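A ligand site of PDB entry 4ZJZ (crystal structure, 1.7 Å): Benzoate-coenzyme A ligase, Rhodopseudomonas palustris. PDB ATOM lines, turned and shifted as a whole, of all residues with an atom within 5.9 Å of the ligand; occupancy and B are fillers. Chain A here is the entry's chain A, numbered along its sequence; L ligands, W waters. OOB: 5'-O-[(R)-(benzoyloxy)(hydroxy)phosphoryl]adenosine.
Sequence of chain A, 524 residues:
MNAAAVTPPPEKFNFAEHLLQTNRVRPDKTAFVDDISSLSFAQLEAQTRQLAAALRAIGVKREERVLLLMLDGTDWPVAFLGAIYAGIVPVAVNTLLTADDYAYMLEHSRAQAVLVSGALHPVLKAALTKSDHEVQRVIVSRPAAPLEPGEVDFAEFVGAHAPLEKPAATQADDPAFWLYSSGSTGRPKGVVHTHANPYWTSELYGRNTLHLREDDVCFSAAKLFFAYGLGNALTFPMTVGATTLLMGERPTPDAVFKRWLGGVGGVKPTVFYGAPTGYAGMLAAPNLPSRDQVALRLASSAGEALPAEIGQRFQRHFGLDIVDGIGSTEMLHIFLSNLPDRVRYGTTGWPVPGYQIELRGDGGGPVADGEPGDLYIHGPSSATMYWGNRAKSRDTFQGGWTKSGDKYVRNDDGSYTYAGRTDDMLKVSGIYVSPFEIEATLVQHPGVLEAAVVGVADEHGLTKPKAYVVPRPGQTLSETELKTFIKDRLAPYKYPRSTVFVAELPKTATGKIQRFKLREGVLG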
ATOM      1  N   SER A 181      11.914 -29.496  26.723  1.00  0.00           N
ATOM      2  CA  SER A 181      11.873 -28.171  26.132  1.00  0.00           C
ATOM      3  C   SER A 181      11.282 -27.220  27.180  1.00  0.00           C
ATOM      4  O   SER A 181      10.431 -27.611  27.945  1.00  0.00           O
ATOM      5  CB  SER A 181      10.924 -28.211  24.957  1.00  0.00           C
ATOM      6  OG  SER A 181      10.942 -26.934  24.276  1.00  0.00           O
ATOM      7  N   PHE A 226      19.670 -31.715  20.965  1.00  0.00           N
ATOM      8  CA  PHE A 226      18.629 -30.891  20.272  1.00  0.00           C
ATOM      9  C   PHE A 226      17.852 -31.828  19.284  1.00  0.00           C
ATOM     10  O   PHE A 226      18.454 -32.636  18.587  1.00  0.00           O
ATOM     11  CB  PHE A 226      19.339 -29.871  19.448  1.00  0.00           C
ATOM     12  CG  PHE A 226      19.901 -28.727  20.265  1.00  0.00           C
ATOM     13  CD1 PHE A 226      19.007 -27.834  20.979  1.00  0.00           C
ATOM     14  CD2 PHE A 226      21.255 -28.553  20.338  1.00  0.00           C
ATOM     15  CE1 PHE A 226      19.551 -26.677  21.735  1.00  0.00           C
ATOM     16  CE2 PHE A 226      21.810 -27.386  20.924  1.00  0.00           C
ATOM     17  CZ  PHE A 226      20.985 -26.485  21.708  1.00  0.00           C
ATOM     18  N   ALA A 227      16.502 -31.678  19.241  1.00  0.00           N
ATOM     19  CA  ALA A 227      15.784 -32.485  18.280  1.00  0.00           C
ATOM     20  C   ALA A 227      16.427 -32.283  16.898  1.00  0.00           C
ATOM     21  O   ALA A 227      16.551 -33.280  16.147  1.00  0.00           O
ATOM     22  CB  ALA A 227      14.327 -31.998  18.299  1.00  0.00           C
ATOM     23  N   TYR A 228      16.864 -31.044  16.595  1.00  0.00           N
ATOM     24  CA  TYR A 228      17.439 -30.787  15.213  1.00  0.00           C
ATOM     25  C   TYR A 228      18.686 -31.668  15.049  1.00  0.00           C
ATOM     26  O   TYR A 228      18.783 -32.411  14.051  1.00  0.00           O
ATOM     27  CB  TYR A 228      17.796 -29.321  15.110  1.00  0.00           C
ATOM     28  CG  TYR A 228      18.361 -28.797  13.790  1.00  0.00           C
ATOM     29  CD1 TYR A 228      17.857 -29.212  12.560  1.00  0.00           C
ATOM     30  CD2 TYR A 228      19.393 -27.931  13.802  1.00  0.00           C
ATOM     31  CE1 TYR A 228      18.371 -28.703  11.388  1.00  0.00           C
ATOM     32  CE2 TYR A 228      19.928 -27.399  12.630  1.00  0.00           C
ATOM     33  CZ  TYR A 228      19.437 -27.795  11.421  1.00  0.00           C
ATOM     34  OH  TYR A 228      19.984 -27.266  10.274  1.00  0.00           O
ATOM     35  N   SER A 301      19.829 -25.210   7.681  1.00  0.00           N
ATOM     36  CA  SER A 301      19.721 -24.373   8.877  1.00  0.00           C
ATOM     37  C   SER A 301      18.339 -24.468   9.523  1.00  0.00           C
ATOM     38  O   SER A 301      17.344 -24.555   8.846  1.00  0.00           O
ATOM     39  CB  SER A 301      20.110 -22.908   8.593  1.00  0.00           C
ATOM     40  OG  SER A 301      19.034 -22.170   7.986  1.00  0.00           O
ATOM     41  N   ALA A 302      18.327 -24.396  10.864  1.00  0.00           N
ATOM     42  CA  ALA A 302      17.063 -24.316  11.584  1.00  0.00           C
ATOM     43  C   ALA A 302      17.370 -23.716  12.940  1.00  0.00           C
ATOM     44  O   ALA A 302      18.575 -23.513  13.348  1.00  0.00           O
ATOM     45  CB  ALA A 302      16.464 -25.696  11.727  1.00  0.00           C
ATOM     46  N   GLY A 303      16.271 -23.545  13.695  1.00  0.00           N
ATOM     47  CA  GLY A 303      16.387 -23.070  15.102  1.00  0.00           C
ATOM     48  C   GLY A 303      15.831 -21.623  15.224  1.00  0.00           C
ATOM     49  O   GLY A 303      15.219 -21.255  16.235  1.00  0.00           O
ATOM     50  N   GLU A 304      16.098 -20.775  14.244  1.00  0.00           N
ATOM     51  CA  GLU A 304      15.625 -19.393  14.223  1.00  0.00           C
ATOM     52  C   GLU A 304      15.465 -19.079  12.712  1.00  0.00           C
ATOM     53  O   GLU A 304      15.992 -19.822  11.862  1.00  0.00           O
ATOM     54  CB  GLU A 304      16.573 -18.391  14.924  1.00  0.00           C
ATOM     55  CG  GLU A 304      17.979 -18.492  14.322  1.00  0.00           C
ATOM     56  CD  GLU A 304      19.044 -17.693  14.996  1.00  0.00           C
ATOM     57  OE1 GLU A 304      18.696 -16.733  15.748  1.00  0.00           O
ATOM     58  OE2 GLU A 304      20.222 -18.108  14.821  1.00  0.00           O
ATOM     59  N   ALA A 305      14.720 -18.013  12.372  1.00  0.00           N
ATOM     60  CA  ALA A 305      14.577 -17.728  10.968  1.00  0.00           C
ATOM     61  C   ALA A 305      15.933 -17.338  10.363  1.00  0.00           C
ATOM     62  O   ALA A 305      16.728 -16.689  11.032  1.00  0.00           O
ATOM     63  CB  ALA A 305      13.500 -16.584  10.711  1.00  0.00           C
ATOM     64  N   LEU A 306      16.226 -17.811   9.130  1.00  0.00           N
ATOM     65  CA  LEU A 306      17.476 -17.450   8.407  1.00  0.00           C
ATOM     66  C   LEU A 306      17.216 -16.049   7.748  1.00  0.00           C
ATOM     67  O   LEU A 306      16.342 -15.874   6.841  1.00  0.00           O
ATOM     68  CB  LEU A 306      17.779 -18.470   7.307  1.00  0.00           C
ATOM     69  CG  LEU A 306      19.046 -18.122   6.432  1.00  0.00           C
ATOM     70  CD1 LEU A 306      20.352 -18.319   7.303  1.00  0.00           C
ATOM     71  CD2 LEU A 306      19.034 -19.107   5.195  1.00  0.00           C
ATOM     72  N   ASP A 324      16.728 -23.471   4.688  1.00  0.00           N
ATOM     73  CA  ASP A 324      16.152 -23.099   6.006  1.00  0.00           C
ATOM     74  C   ASP A 324      14.860 -23.881   6.137  1.00  0.00           C
ATOM     75  O   ASP A 324      14.026 -23.826   5.227  1.00  0.00           O
ATOM     76  CB  ASP A 324      15.910 -21.586   5.953  1.00  0.00           C
ATOM     77  CG  ASP A 324      15.101 -21.030   7.121  1.00  0.00           C
ATOM     78  OD1 ASP A 324      14.847 -21.772   8.100  1.00  0.00           O
ATOM     79  OD2 ASP A 324      14.756 -19.801   7.075  1.00  0.00           O
ATOM     80  N   GLY A 325      14.699 -24.665   7.248  1.00  0.00           N
ATOM     81  CA  GLY A 325      13.365 -25.350   7.482  1.00  0.00           C
ATOM     82  C   GLY A 325      13.104 -25.141   8.999  1.00  0.00           C
ATOM     83  O   GLY A 325      14.051 -24.924   9.833  1.00  0.00           O
ATOM     84  N   ILE A 326      11.831 -25.172   9.371  1.00  0.00           N
ATOM     85  CA  ILE A 326      11.404 -25.065  10.750  1.00  0.00           C
ATOM     86  C   ILE A 326      10.933 -26.401  11.248  1.00  0.00           C
ATOM     87  O   ILE A 326      10.224 -27.091  10.580  1.00  0.00           O
ATOM     88  CB  ILE A 326      10.227 -24.016  10.925  1.00  0.00           C
ATOM     89  CG1 ILE A 326       9.818 -23.993  12.435  1.00  0.00           C
ATOM     90  CG2 ILE A 326       9.077 -24.279   9.993  1.00  0.00           C
ATOM     91  CD1 ILE A 326       8.792 -22.823  12.749  1.00  0.00           C
ATOM     92  N   GLY A 327      11.446 -26.798  12.428  1.00  0.00           N
ATOM     93  CA  GLY A 327      10.971 -27.930  13.142  1.00  0.00           C
ATOM     94  C   GLY A 327      10.815 -27.554  14.605  1.00  0.00           C
ATOM     95  O   GLY A 327      10.984 -26.379  15.000  1.00  0.00           O
ATOM     96  N   SER A 328      10.287 -28.479  15.362  1.00  0.00           N
ATOM     97  CA  SER A 328      10.212 -28.221  16.811  1.00  0.00           C
ATOM     98  C   SER A 328      10.489 -29.531  17.559  1.00  0.00           C
ATOM     99  O   SER A 328      10.412 -30.656  17.008  1.00  0.00           O
ATOM    100  CB  SER A 328       8.799 -27.743  17.163  1.00  0.00           C
ATOM    101  OG  SER A 328       7.832 -28.817  16.952  1.00  0.00           O
ATOM    102  N   THR A 329      10.792 -29.402  18.866  1.00  0.00           N
ATOM    103  CA  THR A 329      10.986 -30.598  19.692  1.00  0.00           C
ATOM    104  C   THR A 329       9.697 -31.407  19.692  1.00  0.00           C
ATOM    105  O   THR A 329       9.750 -32.616  19.558  1.00  0.00           O
ATOM    106  CB  THR A 329      11.308 -30.152  21.131  1.00  0.00           C
ATOM    107  OG1 THR A 329      12.538 -29.352  21.095  1.00  0.00           O
ATOM    108  CG2 THR A 329      11.593 -31.420  21.999  1.00  0.00           C
ATOM    109  N   GLU A 330       8.528 -30.689  19.735  1.00  0.00           N
ATOM    110  CA  GLU A 330       7.226 -31.460  19.722  1.00  0.00           C
ATOM    111  C   GLU A 330       6.957 -32.238  18.430  1.00  0.00           C
ATOM    112  O   GLU A 330       6.359 -33.337  18.496  1.00  0.00           O
ATOM    113  CB  GLU A 330       6.048 -30.493  19.958  1.00  0.00           C
ATOM    114  CG  GLU A 330       6.061 -29.954  21.407  1.00  0.00           C
ATOM    115  CD  GLU A 330       7.031 -28.762  21.687  1.00  0.00           C
ATOM    116  OE1 GLU A 330       7.901 -28.357  20.828  1.00  0.00           O
ATOM    117  OE2 GLU A 330       6.847 -28.155  22.789  1.00  0.00           O
ATOM    118  N   LEU A 332       9.439 -33.228  16.513  1.00  0.00           N
ATOM    119  CA  LEU A 332      10.714 -33.997  16.374  1.00  0.00           C
ATOM    120  C   LEU A 332      11.655 -33.434  15.327  1.00  0.00           C
ATOM    121  O   LEU A 332      12.883 -33.371  15.573  1.00  0.00           O
ATOM    122  CB  LEU A 332      10.455 -35.524  16.240  1.00  0.00           C
ATOM    123  CG  LEU A 332      11.799 -36.348  16.314  1.00  0.00           C
ATOM    124  CD1 LEU A 332      12.482 -36.146  17.707  1.00  0.00           C
ATOM    125  CD2 LEU A 332      11.442 -37.850  16.190  1.00  0.00           C
ATOM    126  N   HIS A 333      11.133 -33.159  14.120  1.00  0.00           N
ATOM    127  CA  HIS A 333      12.089 -32.481  13.167  1.00  0.00           C
ATOM    128  C   HIS A 333      11.330 -31.584  12.236  1.00  0.00           C
ATOM    129  O   HIS A 333      10.235 -31.102  12.578  1.00  0.00           O
ATOM    130  CB  HIS A 333      12.985 -33.502  12.420  1.00  0.00           C
ATOM    131  CG  HIS A 333      14.367 -32.950  12.092  1.00  0.00           C
ATOM    132  ND1 HIS A 333      14.598 -32.261  10.928  1.00  0.00           N
ATOM    133  CD2 HIS A 333      15.574 -33.068  12.736  1.00  0.00           C
ATOM    134  CE1 HIS A 333      15.884 -31.902  10.874  1.00  0.00           C
ATOM    135  NE2 HIS A 333      16.506 -32.419  11.932  1.00  0.00           N
ATOM    136  N   ILE A 334      11.846 -31.336  11.031  1.00  0.00           N
ATOM    137  CA  ILE A 334      11.354 -30.209  10.215  1.00  0.00           C
ATOM    138  C   ILE A 334      10.119 -30.594   9.427  1.00  0.00           C
ATOM    139  O   ILE A 334      10.035 -31.650   8.762  1.00  0.00           O
ATOM    140  CB  ILE A 334      12.480 -29.747   9.263  1.00  0.00           C
ATOM    141  CG1 ILE A 334      13.552 -28.965  10.115  1.00  0.00           C
ATOM    142  CG2 ILE A 334      11.943 -28.848   8.085  1.00  0.00           C
ATOM    143  CD1 ILE A 334      14.944 -28.688   9.344  1.00  0.00           C
ATOM    144  N   THR A 348      10.328 -19.656   4.897  1.00  0.00           N
ATOM    145  CA  THR A 348      10.704 -21.040   5.297  1.00  0.00           C
ATOM    146  C   THR A 348      10.234 -22.112   4.317  1.00  0.00           C
ATOM    147  O   THR A 348      10.067 -23.327   4.699  1.00  0.00           O
ATOM    148  CB  THR A 348      10.200 -21.321   6.768  1.00  0.00           C
ATOM    149  OG1 THR A 348      10.294 -20.081   7.530  1.00  0.00           O
ATOM    150  CG2 THR A 348      11.073 -22.405   7.391  1.00  0.00           C
ATOM    151  N   SER A 404       2.338 -24.780  17.249  1.00  0.00           N
ATOM    152  CA  SER A 404       3.789 -24.520  17.317  1.00  0.00           C
ATOM    153  C   SER A 404       4.173 -23.301  18.142  1.00  0.00           C
ATOM    154  O   SER A 404       5.338 -23.160  18.522  1.00  0.00           O
ATOM    155  CB  SER A 404       4.400 -24.335  15.940  1.00  0.00           C
ATOM    156  OG  SER A 404       3.968 -23.126  15.333  1.00  0.00           O
ATOM    157  N   GLY A 405       3.243 -22.406  18.399  1.00  0.00           N
ATOM    158  CA  GLY A 405       3.685 -21.152  19.083  1.00  0.00           C
ATOM    159  C   GLY A 405       4.299 -20.145  18.129  1.00  0.00           C
ATOM    160  O   GLY A 405       4.863 -19.134  18.542  1.00  0.00           O
ATOM    161  N   ASP A 406       4.218 -20.433  16.846  1.00  0.00           N
ATOM    162  CA  ASP A 406       4.619 -19.442  15.827  1.00  0.00           C
ATOM    163  C   ASP A 406       3.435 -18.847  15.065  1.00  0.00           C
ATOM    164  O   ASP A 406       2.401 -19.499  14.969  1.00  0.00           O
ATOM    165  CB  ASP A 406       5.521 -20.092  14.824  1.00  0.00           C
ATOM    166  CG  ASP A 406       6.782 -20.632  15.508  1.00  0.00           C
ATOM    167  OD1 ASP A 406       7.593 -19.805  16.033  1.00  0.00           O
ATOM    168  OD2 ASP A 406       6.901 -21.853  15.554  1.00  0.00           O
ATOM    169  N   TYR A 408       2.759 -17.260  11.069  1.00  0.00           N
ATOM    170  CA  TYR A 408       3.256 -17.351   9.737  1.00  0.00           C
ATOM    171  C   TYR A 408       2.278 -16.680   8.726  1.00  0.00           C
ATOM    172  O   TYR A 408       1.046 -16.575   8.993  1.00  0.00           O
ATOM    173  CB  TYR A 408       3.434 -18.818   9.305  1.00  0.00           C
ATOM    174  CG  TYR A 408       4.860 -19.286   9.422  1.00  0.00           C
ATOM    175  CD1 TYR A 408       5.744 -19.167   8.348  1.00  0.00           C
ATOM    176  CD2 TYR A 408       5.311 -19.850  10.636  1.00  0.00           C
ATOM    177  CE1 TYR A 408       7.103 -19.612   8.484  1.00  0.00           C
ATOM    178  CE2 TYR A 408       6.645 -20.303  10.799  1.00  0.00           C
ATOM    179  CZ  TYR A 408       7.515 -20.145   9.712  1.00  0.00           C
ATOM    180  OH  TYR A 408       8.822 -20.628   9.790  1.00  0.00           O
ATOM    181  N   TYR A 418       7.937 -16.343   8.010  1.00  0.00           N
ATOM    182  CA  TYR A 418       7.864 -16.316   9.493  1.00  0.00           C
ATOM    183  C   TYR A 418       7.336 -14.961  10.016  1.00  0.00           C
ATOM    184  O   TYR A 418       7.728 -13.901   9.499  1.00  0.00           O
ATOM    185  CB  TYR A 418       9.267 -16.606  10.030  1.00  0.00           C
ATOM    186  CG  TYR A 418       9.299 -16.681  11.545  1.00  0.00           C
ATOM    187  CD1 TYR A 418       8.610 -17.696  12.194  1.00  0.00           C
ATOM    188  CD2 TYR A 418      10.009 -15.734  12.322  1.00  0.00           C
ATOM    189  CE1 TYR A 418       8.609 -17.808  13.539  1.00  0.00           C
ATOM    190  CE2 TYR A 418      10.020 -15.898  13.757  1.00  0.00           C
ATOM    191  CZ  TYR A 418       9.280 -16.967  14.298  1.00  0.00           C
ATOM    192  OH  TYR A 418       9.213 -17.238  15.631  1.00  0.00           O
ATOM    193  N   ARG A 421       6.679 -15.188  17.229  1.00  0.00           N
ATOM    194  CA  ARG A 421       6.063 -16.154  18.141  1.00  0.00           C
ATOM    195  C   ARG A 421       4.774 -15.608  18.734  1.00  0.00           C
ATOM    196  O   ARG A 421       4.568 -14.415  18.766  1.00  0.00           O
ATOM    197  CB  ARG A 421       7.039 -16.509  19.278  1.00  0.00           C
ATOM    198  CG  ARG A 421       8.044 -17.591  18.756  1.00  0.00           C
ATOM    199  CD  ARG A 421       8.722 -18.383  19.683  1.00  0.00           C
ATOM    200  NE  ARG A 421       7.865 -19.118  20.644  1.00  0.00           N
ATOM    201  CZ  ARG A 421       7.609 -20.410  20.530  1.00  0.00           C
ATOM    202  NH1 ARG A 421       8.073 -21.114  19.463  1.00  0.00           N
ATOM    203  NH2 ARG A 421       6.909 -21.006  21.513  1.00  0.00           N
ATOM    204  N   LYS A 427      14.397 -16.916  20.329  1.00  0.00           N
ATOM    205  CA  LYS A 427      15.335 -17.929  19.943  1.00  0.00           C
ATOM    206  C   LYS A 427      16.560 -17.146  19.623  1.00  0.00           C
ATOM    207  O   LYS A 427      16.573 -16.365  18.654  1.00  0.00           O
ATOM    208  CB  LYS A 427      14.843 -18.660  18.621  1.00  0.00           C
ATOM    209  CG  LYS A 427      13.814 -19.841  18.908  1.00  0.00           C
ATOM    210  CD  LYS A 427      14.526 -20.807  19.821  1.00  0.00           C
ATOM    211  CE  LYS A 427      14.027 -22.268  19.755  1.00  0.00           C
ATOM    212  NZ  LYS A 427      14.645 -22.918  18.526  1.00  0.00           N
ATOM    213  N   GLY A 430      19.403 -19.507  17.641  1.00  0.00           N
ATOM    214  CA  GLY A 430      18.481 -20.632  17.370  1.00  0.00           C
ATOM    215  C   GLY A 430      18.162 -21.504  18.617  1.00  0.00           C
ATOM    216  O   GLY A 430      17.671 -22.596  18.498  1.00  0.00           O
ATOM    217  N   ILE A 431      18.371 -21.014  19.855  1.00  0.00           N
ATOM    218  CA  ILE A 431      18.120 -21.829  21.108  1.00  0.00           C
ATOM    219  C   ILE A 431      17.111 -21.026  22.024  1.00  0.00           C
ATOM    220  O   ILE A 431      17.217 -19.817  22.042  1.00  0.00           O
ATOM    221  CB  ILE A 431      19.398 -21.985  21.919  1.00  0.00           C
ATOM    222  CG1 ILE A 431      20.419 -22.669  21.020  1.00  0.00           C
ATOM    223  CG2 ILE A 431      19.093 -22.802  23.221  1.00  0.00           C
ATOM    224  CD1 ILE A 431      21.867 -22.676  21.703  1.00  0.00           C
ATOM    225  N   TYR A 432      16.177 -21.672  22.742  1.00  0.00           N
ATOM    226  CA  TYR A 432      15.190 -20.883  23.519  1.00  0.00           C
ATOM    227  C   TYR A 432      15.836 -20.090  24.655  1.00  0.00           C
ATOM    228  O   TYR A 432      16.673 -20.622  25.403  1.00  0.00           O
ATOM    229  CB  TYR A 432      14.185 -21.851  24.144  1.00  0.00           C
ATOM    230  CG  TYR A 432      12.986 -22.199  23.336  1.00  0.00           C
ATOM    231  CD1 TYR A 432      12.244 -21.217  22.646  1.00  0.00           C
ATOM    232  CD2 TYR A 432      12.625 -23.555  23.209  1.00  0.00           C
ATOM    233  CE1 TYR A 432      11.083 -21.594  21.855  1.00  0.00           C
ATOM    234  CE2 TYR A 432      11.513 -23.942  22.434  1.00  0.00           C
ATOM    235  CZ  TYR A 432      10.751 -22.956  21.801  1.00  0.00           C
ATOM    236  OH  TYR A 432       9.665 -23.329  21.061  1.00  0.00           O
HETATM  237  C1  OOB L   1      13.937 -26.550  17.015  1.00  0.00           C
HETATM  238  O1  OOB L   1      13.191 -26.980  18.190  1.00  0.00           O
HETATM  239  P1  OOB L   1      12.742 -26.100  19.517  1.00  0.00           P
HETATM  240  O2  OOB L   1      11.732 -26.902  20.102  1.00  0.00           O
HETATM  241  O3  OOB L   1      14.114 -25.753  20.139  1.00  0.00           O
HETATM  242  O4  OOB L   1      12.187 -24.712  18.983  1.00  0.00           O
HETATM  243  C2  OOB L   1      11.136 -24.673  17.986  1.00  0.00           C
HETATM  244  C3  OOB L   1      10.837 -23.245  17.618  1.00  0.00           C
HETATM  245  C4  OOB L   1       9.742 -23.081  16.547  1.00  0.00           C
HETATM  246  O5  OOB L   1       8.418 -23.152  17.159  1.00  0.00           O
HETATM  247  C5  OOB L   1      10.134 -21.668  16.105  1.00  0.00           C
HETATM  248  O6  OOB L   1       9.716 -20.572  16.986  1.00  0.00           O
HETATM  249  C6  OOB L   1      11.661 -21.703  16.147  1.00  0.00           C
HETATM  250  O7  OOB L   1      12.033 -22.587  17.139  1.00  0.00           O
HETATM  251  N1  OOB L   1      12.230 -22.221  14.894  1.00  0.00           N
HETATM  252  C7  OOB L   1      12.229 -21.467  13.811  1.00  0.00           C
HETATM  253  C8  OOB L   1      12.944 -22.251  12.810  1.00  0.00           C
HETATM  254  N2  OOB L   1      13.346 -23.488  13.341  1.00  0.00           N
HETATM  255  C9  OOB L   1      12.940 -23.399  14.645  1.00  0.00           C
HETATM  256  N3  OOB L   1      11.727 -20.184  13.475  1.00  0.00           N
HETATM  257  C10 OOB L   1      11.872 -19.754  12.211  1.00  0.00           C
HETATM  258  N4  OOB L   1      12.536 -20.386  11.245  1.00  0.00           N
HETATM  259  C11 OOB L   1      13.052 -21.621  11.477  1.00  0.00           C
HETATM  260  N5  OOB L   1      13.756 -22.279  10.560  1.00  0.00           N
HETATM  261  O8  OOB L   1      14.370 -25.381  16.856  1.00  0.00           O
HETATM  262  C12 OOB L   1      14.024 -27.567  15.909  1.00  0.00           C
HETATM  263  C13 OOB L   1      14.476 -27.103  14.667  1.00  0.00           C
HETATM  264  C14 OOB L   1      14.588 -28.059  13.627  1.00  0.00           C
HETATM  265  C15 OOB L   1      14.353 -29.434  13.879  1.00  0.00           C
HETATM  266  C16 OOB L   1      13.918 -29.879  15.164  1.00  0.00           C
HETATM  267  C17 OOB L   1      13.769 -28.919  16.182  1.00  0.00           C
HETATM  268  O   HOH W   1       7.145 -25.176  18.771  1.00  0.00           O
HETATM  269  O   HOH W   2      12.535 -19.441   8.638  1.00  0.00           O
HETATM  270  O   HOH W   3      15.911 -24.618  22.539  1.00  0.00           O
HETATM  271  O   HOH W   4       9.380 -26.015  20.601  1.00  0.00           O
HETATM  272  O   HOH W   5      11.766 -18.173  15.678  1.00  0.00           O
HETATM  273  O   HOH W   6      16.347 -28.598  18.202  1.00  0.00           O
HETATM  274  O   HOH W   7      17.051 -21.443   9.772  1.00  0.00           O
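Water W4 lies within hydrogen-bond range of O2 of the ligand (2.6 Å), OH of Tyr 432 (2.7 Å) and OE1 of Glu 330 (2.8 Å).
Water W2 lies within hydrogen-bond range of the side-chain hydroxyl (OG1) of Thr 348, the side-chain carboxylate (OD2) of Asp 324 and a nitrogen (N4) of the ligand.
Water W1 bridges the backbone carbonyl oxygen (O) of Ser 404 (2.7 Å) and an oxygen (O5) of the ligand (2.9 Å).
Water W5 bridges the side-chain hydroxyl of Tyr 418 and a nitrogen (N3) of the ligand.
Water W3 lies within hydrogen-bond range of N of Tyr 432 and O3 of the ligand.
Water W7 lies within hydrogen-bond range of the side-chain hydroxyl (OG) of Ser 301, the side-chain carboxylate (OD1) of Asp 324, the backbone carbonyl oxygen (O) of Glu 304, the backbone NH (N) of Ala 302 and a nitrogen (N5) of the ligand.
The backbone NH (N) of Asp 406 is in hydrogen-bond range of the side-chain hydroxyl (OG) of Ser 404 (3.1 Å).
The backbone carbonyl oxygen (O) of Gly 303 is in hydrogen-bond range of the side-chain amino group (NZ) of Lys 427 (2.9 Å).
NZ of Lys 427 sits at hydrogen-bond distance from O of Gly 430 (3.0 Å).
The backbone NH (N) of Gly 430 lies close to the side-chain carboxylate (OE2) of Glu 304 (3.3 Å).
The backbone NH of Ala 302 sits at hydrogen-bond distance from the side-chain hydroxyl of Tyr 228 (3.4 Å).
The backbone carbonyl oxygen of Tyr 228 is in hydrogen-bond range of a ring nitrogen (NE2) of His 333, 3.1 Å away.
OH of Tyr 228 sits close to N of Ser 301 (3.3 Å).
OH of Tyr 408 sits at hydrogen-bond distance from OG1 of Thr 348.
An oxygen (O6) of the ligand is in hydrogen-bond range of the side-chain carboxylate (OD1) of Asp 406 (2.5 Å).
The side-chain carboxylate of Asp 324 sits at hydrogen-bond distance from a nitrogen (N5) of the ligand (2.7 Å).
O of Gly 325 lies within hydrogen-bond range of N5 of the ligand (2.8 Å).
N of Thr 329 sits at hydrogen-bond distance from O2 of the ligand (2.9 Å).
The side-chain hydroxyl (OG1) of Thr 329 sits at hydrogen-bond distance from an oxygen (O2) of the ligand, 2.8 Å away.
N2 of the ligand lies within hydrogen-bond range of N of Gly 303 (2.9 Å).
An oxygen (O3) of the ligand is in salt-bridge range of the side-chain amino group (NZ) of Lys 427 (3.3 Å).
O6 of the ligand is in hydrogen-bond range of NH1 of Arg 421, 3.0 Å away.
N of Ala 305 sits close to N4 of the ligand, 3.4 Å away.
An oxygen (O5) of the ligand sits at hydrogen-bond distance from the backbone carbonyl oxygen (O) of Ser 404 (3.4 Å).
Residues that only touch the ligand: Gly 327 (3.4 Å), Glu 304 (3.5 Å), Tyr 228 (3.5 Å), Ser 328 (3.5 Å), Tyr 432 (3.5 Å), Ala 302 (3.6 Å), Ile 326 (3.6 Å), Tyr 418 (3.6 Å), Leu 332 (3.7 Å), His 333 (3.8 Å), Ile 334 (3.8 Å), Ala 227 (3.8 Å) and Tyr 408 (3.99 Å).
22 residues have an atom within 4 Å of the ligand: Ala 227, Tyr 228, Ala 302, Gly 303, Glu 304, Ala 305, Asp 324, Gly 325, Ile 326, Gly 327, Ser 328, Thr 329, Leu 332, His 333, Ile 334, Ser 404, Asp 406, Tyr 408, Tyr 418, Arg 421, Lys 427 and Tyr 432.
The nearest printed residue that does not touch the ligand is Thr 348 (4.2 Å).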
